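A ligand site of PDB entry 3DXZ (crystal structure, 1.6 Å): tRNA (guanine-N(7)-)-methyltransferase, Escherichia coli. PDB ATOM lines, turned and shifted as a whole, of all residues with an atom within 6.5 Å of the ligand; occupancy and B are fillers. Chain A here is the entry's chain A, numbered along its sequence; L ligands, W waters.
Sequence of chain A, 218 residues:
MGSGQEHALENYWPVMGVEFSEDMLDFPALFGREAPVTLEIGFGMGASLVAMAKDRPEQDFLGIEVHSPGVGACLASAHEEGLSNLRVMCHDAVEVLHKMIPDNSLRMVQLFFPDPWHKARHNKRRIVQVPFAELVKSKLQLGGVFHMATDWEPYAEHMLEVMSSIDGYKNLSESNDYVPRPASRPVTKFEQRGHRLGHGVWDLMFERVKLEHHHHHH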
ATOM      1  N   GLU A  40      10.076 -10.697   6.690  1.00  0.00           N
ATOM      2  CA  GLU A  40      10.753 -11.645   5.798  1.00  0.00           C
ATOM      3  C   GLU A  40       9.837 -12.002   4.640  1.00  0.00           C
ATOM      4  O   GLU A  40       8.721 -12.494   4.859  1.00  0.00           O
ATOM      5  CB  GLU A  40      11.214 -12.926   6.493  1.00  0.00           C
ATOM      6  CG  GLU A  40      12.010 -13.792   5.507  1.00  0.00           C
ATOM      7  CD  GLU A  40      12.499 -15.113   6.066  1.00  0.00           C
ATOM      8  OE1 GLU A  40      12.246 -15.430   7.243  1.00  0.00           O
ATOM      9  OE2 GLU A  40      13.145 -15.854   5.287  1.00  0.00           O
ATOM     10  N   ILE A  41      10.329 -11.751   3.432  1.00  0.00           N
ATOM     11  CA  ILE A  41       9.613 -12.088   2.207  1.00  0.00           C
ATOM     12  C   ILE A  41      10.075 -13.450   1.693  1.00  0.00           C
ATOM     13  O   ILE A  41      11.269 -13.711   1.556  1.00  0.00           O
ATOM     14  CB  ILE A  41       9.825 -11.018   1.123  1.00  0.00           C
ATOM     15  CG1 ILE A  41       9.232  -9.688   1.582  1.00  0.00           C
ATOM     16  CG2 ILE A  41       9.194 -11.464  -0.206  1.00  0.00           C
ATOM     17  CD1 ILE A  41       9.605  -8.478   0.735  1.00  0.00           C
ATOM     18  N   GLY A  42       9.109 -14.326   1.399  1.00  0.00           N
ATOM     19  CA  GLY A  42       9.398 -15.665   0.882  1.00  0.00           C
ATOM     20  C   GLY A  42      10.130 -16.523   1.878  1.00  0.00           C
ATOM     21  O   GLY A  42      11.188 -17.091   1.584  1.00  0.00           O
ATOM     22  N   PHE A  43       9.549 -16.636   3.071  1.00  0.00           N
ATOM     23  CA  PHE A  43      10.209 -17.308   4.188  1.00  0.00           C
ATOM     24  C   PHE A  43      10.293 -18.835   4.081  1.00  0.00           C
ATOM     25  O   PHE A  43      10.935 -19.473   4.909  1.00  0.00           O
ATOM     26  CB  PHE A  43       9.579 -16.882   5.527  1.00  0.00           C
ATOM     27  CG  PHE A  43       8.111 -17.223   5.664  1.00  0.00           C
ATOM     28  CD1 PHE A  43       7.693 -18.545   5.795  1.00  0.00           C
ATOM     29  CD2 PHE A  43       7.167 -16.215   5.729  1.00  0.00           C
ATOM     30  CE1 PHE A  43       6.337 -18.861   5.951  1.00  0.00           C
ATOM     31  CE2 PHE A  43       5.811 -16.500   5.890  1.00  0.00           C
ATOM     32  CZ  PHE A  43       5.392 -17.837   5.997  1.00  0.00           C
ATOM     33  N   GLY A  44       9.655 -19.408   3.060  1.00  0.00           N
ATOM     34  CA  GLY A  44       9.689 -20.849   2.844  1.00  0.00           C
ATOM     35  C   GLY A  44       8.996 -21.589   3.974  1.00  0.00           C
ATOM     36  O   GLY A  44       7.830 -21.330   4.262  1.00  0.00           O
ATOM     37  N   MET A  45       9.733 -22.494   4.630  1.00  0.00           N
ATOM     38  CA  MET A  45       9.195 -23.250   5.760  1.00  0.00           C
ATOM     39  C   MET A  45       9.277 -22.455   7.062  1.00  0.00           C
ATOM     40  O   MET A  45       8.779 -22.896   8.090  1.00  0.00           O
ATOM     41  CB  MET A  45       9.909 -24.604   5.906  1.00  0.00           C
ATOM     42  CG  MET A  45       9.775 -25.485   4.671  1.00  0.00           C
ATOM     43  SD  MET A  45       8.077 -26.012   4.360  1.00  0.00           S
ATOM     44  CE  MET A  45       8.133 -26.227   2.579  1.00  0.00           C
ATOM     45  N   GLY A  46       9.901 -21.278   7.002  1.00  0.00           N
ATOM     46  CA  GLY A  46       9.920 -20.345   8.127  1.00  0.00           C
ATOM     47  C   GLY A  46      10.941 -20.576   9.224  1.00  0.00           C
ATOM     48  O   GLY A  46      10.833 -19.974  10.284  1.00  0.00           O
ATOM     49  N   SER A  48      14.141 -19.714   9.508  1.00  0.00           N
ATOM     50  CA  SER A  48      14.854 -18.476   9.832  1.00  0.00           C
ATOM     51  C   SER A  48      13.968 -17.525  10.627  1.00  0.00           C
ATOM     52  O   SER A  48      14.396 -16.973  11.649  1.00  0.00           O
ATOM     53  CB  SER A  48      15.355 -17.802   8.555  1.00  0.00           C
ATOM     54  OG  SER A  48      16.095 -16.639   8.882  1.00  0.00           O
ATOM     55  N   ILE A  64       5.841 -13.162   4.867  1.00  0.00           N
ATOM     56  CA  ILE A  64       4.923 -13.330   3.731  1.00  0.00           C
ATOM     57  C   ILE A  64       5.434 -14.451   2.834  1.00  0.00           C
ATOM     58  O   ILE A  64       6.602 -14.440   2.449  1.00  0.00           O
ATOM     59  CB  ILE A  64       4.800 -12.041   2.883  1.00  0.00           C
ATOM     60  CG1 ILE A  64       4.404 -10.844   3.766  1.00  0.00           C
ATOM     61  CG2 ILE A  64       3.779 -12.247   1.770  1.00  0.00           C
ATOM     62  CD1 ILE A  64       4.643  -9.507   3.100  1.00  0.00           C
ATOM     63  N   GLU A  65       4.567 -15.401   2.497  1.00  0.00           N
ATOM     64  CA  GLU A  65       4.958 -16.549   1.683  1.00  0.00           C
ATOM     65  C   GLU A  65       3.748 -17.057   0.902  1.00  0.00           C
ATOM     66  O   GLU A  65       2.722 -17.385   1.522  1.00  0.00           O
ATOM     67  CB  GLU A  65       5.544 -17.652   2.593  1.00  0.00           C
ATOM     68  CG  GLU A  65       5.892 -18.994   1.965  1.00  0.00           C
ATOM     69  CD  GLU A  65       6.797 -18.849   0.755  1.00  0.00           C
ATOM     70  OE1 GLU A  65       8.021 -18.669   0.931  1.00  0.00           O
ATOM     71  OE2 GLU A  65       6.246 -18.909  -0.363  1.00  0.00           O
ATOM     72  N   VAL A  66       3.866 -17.103  -0.421  1.00  0.00           N
ATOM     73  CA  VAL A  66       2.772 -17.568  -1.304  1.00  0.00           C
ATOM     74  C   VAL A  66       2.553 -19.087  -1.237  1.00  0.00           C
ATOM     75  O   VAL A  66       1.478 -19.575  -1.612  1.00  0.00           O
ATOM     76  CB  VAL A  66       2.983 -17.173  -2.788  1.00  0.00           C
ATOM     77  CG1 VAL A  66       2.763 -15.682  -2.978  1.00  0.00           C
ATOM     78  CG2 VAL A  66       4.359 -17.604  -3.300  1.00  0.00           C
ATOM     79  N   HIS A  67       3.572 -19.801  -0.797  1.00  0.00           N
ATOM     80  CA  HIS A  67       3.545 -21.261  -0.729  1.00  0.00           C
ATOM     81  C   HIS A  67       2.842 -21.681   0.559  1.00  0.00           C
ATOM     82  O   HIS A  67       3.435 -21.606   1.649  1.00  0.00           O
ATOM     83  CB  HIS A  67       4.971 -21.806  -0.793  1.00  0.00           C
ATOM     84  CG  HIS A  67       5.058 -23.303  -0.852  1.00  0.00           C
ATOM     85  ND1 HIS A  67       4.559 -24.041  -1.902  1.00  0.00           N
ATOM     86  CD2 HIS A  67       5.621 -24.191  -0.002  1.00  0.00           C
ATOM     87  CE1 HIS A  67       4.793 -25.328  -1.684  1.00  0.00           C
ATOM     88  NE2 HIS A  67       5.438 -25.445  -0.534  1.00  0.00           N
ATOM     89  N   HIS A  91       0.217 -14.591   0.573  1.00  0.00           N
ATOM     90  CA  HIS A  91      -0.171 -13.656  -0.468  1.00  0.00           C
ATOM     91  C   HIS A  91       1.091 -13.139  -1.149  1.00  0.00           C
ATOM     92  O   HIS A  91       2.181 -13.221  -0.571  1.00  0.00           O
ATOM     93  CB  HIS A  91      -0.944 -12.474   0.122  1.00  0.00           C
ATOM     94  CG  HIS A  91      -1.816 -11.775  -0.881  1.00  0.00           C
ATOM     95  ND1 HIS A  91      -1.405 -10.667  -1.581  1.00  0.00           N
ATOM     96  CD2 HIS A  91      -3.075 -12.038  -1.287  1.00  0.00           C
ATOM     97  CE1 HIS A  91      -2.382 -10.273  -2.391  1.00  0.00           C
ATOM     98  NE2 HIS A  91      -3.408 -11.082  -2.220  1.00  0.00           N
ATOM     99  N   ASP A  92       0.937 -12.630  -2.371  1.00  0.00           N
ATOM    100  CA  ASP A  92       2.030 -12.005  -3.101  1.00  0.00           C
ATOM    101  C   ASP A  92       2.582 -10.826  -2.293  1.00  0.00           C
ATOM    102  O   ASP A  92       1.858  -9.861  -2.021  1.00  0.00           O
ATOM    103  CB  ASP A  92       1.561 -11.552  -4.485  1.00  0.00           C
ATOM    104  CG  ASP A  92       2.489 -10.532  -5.129  1.00  0.00           C
ATOM    105  OD1 ASP A  92       3.729 -10.688  -5.051  1.00  0.00           O
ATOM    106  OD2 ASP A  92       1.970  -9.566  -5.737  1.00  0.00           O
ATOM    107  N   ALA A  93       3.861 -10.892  -1.930  1.00  0.00           N
ATOM    108  CA  ALA A  93       4.464  -9.856  -1.085  1.00  0.00           C
ATOM    109  C   ALA A  93       4.450  -8.469  -1.725  1.00  0.00           C
ATOM    110  O   ALA A  93       4.368  -7.465  -1.025  1.00  0.00           O
ATOM    111  CB  ALA A  93       5.874 -10.240  -0.687  1.00  0.00           C
ATOM    112  N   VAL A  94       4.551  -8.411  -3.054  1.00  0.00           N
ATOM    113  CA  VAL A  94       4.544  -7.120  -3.752  1.00  0.00           C
ATOM    114  C   VAL A  94       3.236  -6.384  -3.472  1.00  0.00           C
ATOM    115  O   VAL A  94       3.260  -5.201  -3.112  1.00  0.00           O
ATOM    116  CB  VAL A  94       4.784  -7.298  -5.258  1.00  0.00           C
ATOM    117  CG1 VAL A  94       4.746  -5.950  -5.973  1.00  0.00           C
ATOM    118  CG2 VAL A  94       6.107  -7.997  -5.486  1.00  0.00           C
ATOM    119  N   LEU A 111      15.214 -11.071   2.546  1.00  0.00           N
ATOM    120  CA  LEU A 111      14.861 -11.828   1.348  1.00  0.00           C
ATOM    121  C   LEU A 111      15.944 -12.857   1.102  1.00  0.00           C
ATOM    122  O   LEU A 111      16.960 -12.564   0.463  1.00  0.00           O
ATOM    123  CB  LEU A 111      14.693 -10.883   0.159  1.00  0.00           C
ATOM    124  CG  LEU A 111      14.251 -11.519  -1.163  1.00  0.00           C
ATOM    125  CD1 LEU A 111      12.753 -11.795  -1.167  1.00  0.00           C
ATOM    126  CD2 LEU A 111      14.645 -10.605  -2.317  1.00  0.00           C
ATOM    127  N   PHE A 112      15.720 -14.057   1.630  1.00  0.00           N
ATOM    128  CA  PHE A 112      16.746 -15.106   1.628  1.00  0.00           C
ATOM    129  C   PHE A 112      16.464 -16.172   0.588  1.00  0.00           C
ATOM    130  O   PHE A 112      15.385 -16.788   0.564  1.00  0.00           O
ATOM    131  CB  PHE A 112      16.875 -15.734   3.020  1.00  0.00           C
ATOM    132  CG  PHE A 112      17.260 -14.747   4.121  1.00  0.00           C
ATOM    133  CD1 PHE A 112      17.997 -13.593   3.833  1.00  0.00           C
ATOM    134  CD2 PHE A 112      16.896 -15.011   5.439  1.00  0.00           C
ATOM    135  CE1 PHE A 112      18.367 -12.713   4.860  1.00  0.00           C
ATOM    136  CE2 PHE A 112      17.259 -14.143   6.483  1.00  0.00           C
ATOM    137  CZ  PHE A 112      17.998 -12.987   6.185  1.00  0.00           C
ATOM    138  N   PHE A 113      17.444 -16.368  -0.292  1.00  0.00           N
ATOM    139  CA  PHE A 113      17.365 -17.334  -1.384  1.00  0.00           C
ATOM    140  C   PHE A 113      16.104 -17.187  -2.227  1.00  0.00           C
ATOM    141  O   PHE A 113      15.385 -18.162  -2.474  1.00  0.00           O
ATOM    142  CB  PHE A 113      17.622 -18.756  -0.863  1.00  0.00           C
ATOM    143  CG  PHE A 113      18.884 -18.835  -0.080  1.00  0.00           C
ATOM    144  CD1 PHE A 113      20.105 -18.914  -0.730  1.00  0.00           C
ATOM    145  CD2 PHE A 113      18.879 -18.712   1.312  1.00  0.00           C
ATOM    146  CE1 PHE A 113      21.300 -18.936  -0.004  1.00  0.00           C
ATOM    147  CE2 PHE A 113      20.065 -18.723   2.049  1.00  0.00           C
ATOM    148  CZ  PHE A 113      21.276 -18.838   1.380  1.00  0.00           C
ATOM    149  N   PRO A 114      15.840 -15.947  -2.699  1.00  0.00           N
ATOM    150  CA  PRO A 114      14.670 -15.792  -3.562  1.00  0.00           C
ATOM    151  C   PRO A 114      14.866 -16.605  -4.837  1.00  0.00           C
ATOM    152  O   PRO A 114      16.018 -16.880  -5.215  1.00  0.00           O
ATOM    153  CB  PRO A 114      14.672 -14.298  -3.869  1.00  0.00           C
ATOM    154  CG  PRO A 114      16.108 -13.856  -3.714  1.00  0.00           C
ATOM    155  CD  PRO A 114      16.611 -14.691  -2.568  1.00  0.00           C
ATOM    156  N   ASP A 115      13.768 -17.001  -5.471  1.00  0.00           N
ATOM    157  CA  ASP A 115      13.808 -17.876  -6.645  1.00  0.00           C
ATOM    158  C   ASP A 115      14.886 -17.372  -7.608  1.00  0.00           C
ATOM    159  O   ASP A 115      14.827 -16.242  -8.065  1.00  0.00           O
ATOM    160  CB  ASP A 115      12.439 -17.914  -7.348  1.00  0.00           C
ATOM    161  CG  ASP A 115      11.331 -18.477  -6.454  1.00  0.00           C
ATOM    162  OD1 ASP A 115      11.623 -19.345  -5.609  1.00  0.00           O
ATOM    163  OD2 ASP A 115      10.160 -18.066  -6.607  1.00  0.00           O
ATOM    164  N   ILE A 127      12.679 -11.511  -8.416  1.00  0.00           N
ATOM    165  CA  ILE A 127      11.956 -10.481  -7.665  1.00  0.00           C
ATOM    166  C   ILE A 127      12.782  -9.211  -7.446  1.00  0.00           C
ATOM    167  O   ILE A 127      12.221  -8.118  -7.376  1.00  0.00           O
ATOM    168  CB  ILE A 127      11.398 -11.013  -6.323  1.00  0.00           C
ATOM    169  CG1 ILE A 127      10.293 -10.102  -5.792  1.00  0.00           C
ATOM    170  CG2 ILE A 127      12.530 -11.230  -5.292  1.00  0.00           C
ATOM    171  CD1 ILE A 127       9.504 -10.684  -4.655  1.00  0.00           C
ATOM    172  N   THR A 188      22.918 -22.271   5.985  1.00  0.00           N
ATOM    173  CA  THR A 188      22.191 -23.324   5.275  1.00  0.00           C
ATOM    174  C   THR A 188      22.879 -24.654   5.575  1.00  0.00           C
ATOM    175  O   THR A 188      24.008 -24.663   6.071  1.00  0.00           O
ATOM    176  CB  THR A 188      22.126 -23.100   3.742  1.00  0.00           C
ATOM    177  OG1 THR A 188      23.385 -23.449   3.136  1.00  0.00           O
ATOM    178  CG2 THR A 188      21.784 -21.660   3.392  1.00  0.00           C
HETATM  179  N1  LIG L   1      13.741 -18.213   2.403  1.00  0.00           N
HETATM  180  C1  LIG L   1      13.404 -19.654   2.302  1.00  0.00           C
HETATM  181  C2  LIG L   1      12.738 -19.990   0.964  1.00  0.00           C
HETATM  182  C3  LIG L   1      13.583 -19.691  -0.273  1.00  0.00           C
HETATM  183  S1  LIG L   1      12.732 -20.206  -1.788  1.00  0.00           S
HETATM  184  C4  LIG L   1      14.663 -20.490   2.451  1.00  0.00           C
HETATM  185  O1  LIG L   1      15.784 -19.948   2.378  1.00  0.00           O
HETATM  186  O2  LIG L   1      14.575 -21.708   2.621  1.00  0.00           O
HETATM  187  C5  LIG L   1      11.982 -18.601  -2.167  1.00  0.00           C
HETATM  188  C6  LIG L   1      10.567 -18.455  -1.631  1.00  0.00           C
HETATM  189  O3  LIG L   1      10.004 -17.227  -2.067  1.00  0.00           O
HETATM  190  C7  LIG L   1       9.612 -19.560  -2.098  1.00  0.00           C
HETATM  191  O4  LIG L   1       9.068 -20.246  -0.978  1.00  0.00           O
HETATM  192  C8  LIG L   1       8.530 -18.815  -2.890  1.00  0.00           C
HETATM  193  O5  LIG L   1       7.211 -19.318  -2.769  1.00  0.00           O
HETATM  194  C9  LIG L   1       8.629 -17.426  -2.279  1.00  0.00           C
HETATM  195  N2  LIG L   1       8.130 -16.354  -3.124  1.00  0.00           N
HETATM  196  C10 LIG L   1       8.459 -16.093  -4.429  1.00  0.00           C
HETATM  197  N3  LIG L   1       7.791 -14.987  -4.806  1.00  0.00           N
HETATM  198  C11 LIG L   1       7.053 -14.517  -3.773  1.00  0.00           C
HETATM  199  C12 LIG L   1       6.197 -13.430  -3.612  1.00  0.00           C
HETATM  200  N4  LIG L   1       5.947 -12.571  -4.606  1.00  0.00           N
HETATM  201  N5  LIG L   1       5.573 -13.224  -2.393  1.00  0.00           N
HETATM  202  C13 LIG L   1       5.801 -14.090  -1.343  1.00  0.00           C
HETATM  203  N6  LIG L   1       6.649 -15.165  -1.493  1.00  0.00           N
HETATM  204  C14 LIG L   1       7.271 -15.366  -2.691  1.00  0.00           C
HETATM  205  O   HOH W   1      16.855 -22.083   0.780  1.00  0.00           O
HETATM  206  O   HOH W   2      13.353 -15.044   2.775  1.00  0.00           O
HETATM  207  O   HOH W   3      14.601 -18.081   5.119  1.00  0.00           O
HETATM  208  O   HOH W   4      16.282 -23.172   3.974  1.00  0.00           O
HETATM  209  O   HOH W   5       6.352 -21.015  -4.672  1.00  0.00           O
HETATM  210  O   HOH W   6      17.316 -18.712   4.564  1.00  0.00           O
HETATM  211  O   HOH W   7       9.402 -14.038  -6.944  1.00  0.00           O
HETATM  212  O   HOH W   8      10.041 -22.740  -0.240  1.00  0.00           O
HETATM  213  O   HOH W   9       6.792 -12.395  -7.403  1.00  0.00           O
HETATM  214  O   HOH W  10      12.429 -23.092   3.526  1.00  0.00           O
HETATM  215  O   HOH W  11      11.416 -14.809  -2.617  1.00  0.00           O
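The backbone carbonyl oxygen (O) of Gly 42 is in hydrogen-bond range of a nitrogen (N1) of the ligand (2.9 Å).
The backbone NH (N) of Ala 93 sits at hydrogen-bond distance from a nitrogen (N5) of the ligand (2.9 Å).
O5 of the ligand sits at hydrogen-bond distance from OE2 of Glu 65, 2.6 Å away.
A nitrogen (N1) of the ligand is in salt-bridge range of the side-chain carboxylate (OE2) of Glu 40 (3.8 Å).
A nitrogen (N4) of the ligand lies within hydrogen-bond range of the side-chain carboxylate (OD1) of Asp 92.
The backbone carbonyl oxygen (O) of Phe 112 is in hydrogen-bond range of a nitrogen (N1) of the ligand (2.8 Å).
OD1 of Asp 92 sits at hydrogen-bond distance from N of Val 94 (3.1 Å).
OE2 of Glu 65 lies within hydrogen-bond range of N of His 67 (2.9 Å).
N of Gly 42 is in hydrogen-bond range of O of Ile 64, at 2.7 Å.
The side-chain carboxylate (OE1) of Glu 65 lies within hydrogen-bond range of the backbone NH (N) of Phe 43 (3.3 Å).
The side-chain carboxylate of Glu 65 is in hydrogen-bond range of the backbone NH of Gly 44, at 2.8 Å.
O of Glu 40 lies within hydrogen-bond range of N of Ile 64, 3.0 Å away.
O of Phe 113 sits close to S1 of the ligand.
Phe 43 touches the ligand.
Gly 44 touches the ligand (CA to C2, 3.7 Å).
Ile 64 touches the ligand.
CG2 of Val 66 touches O5 of the ligand (3.4 Å).
His 67 touches the ligand.
His 91 touches the ligand (O to C13, 3.8 Å).
Asp 115 touches the ligand (OD2 to C10, 3.4 Å).
Hydrophobic or aromatic side chains that line the ligand: Val 66, His 67, Ala 93 and Phe 113.
Of the 23 residues printed, 14 come within 4 Å of the ligand.
The nearest printed residue that does not touch the ligand is Ile 127 (4.03 Å).
Water W10 lies within hydrogen-bond range of O2 of the ligand (2.7 Å) and N of Met 45 (3.0 Å).
Water W3 bridges OE2 of Glu 40 (2.7 Å) and N1 of the ligand (2.9 Å).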
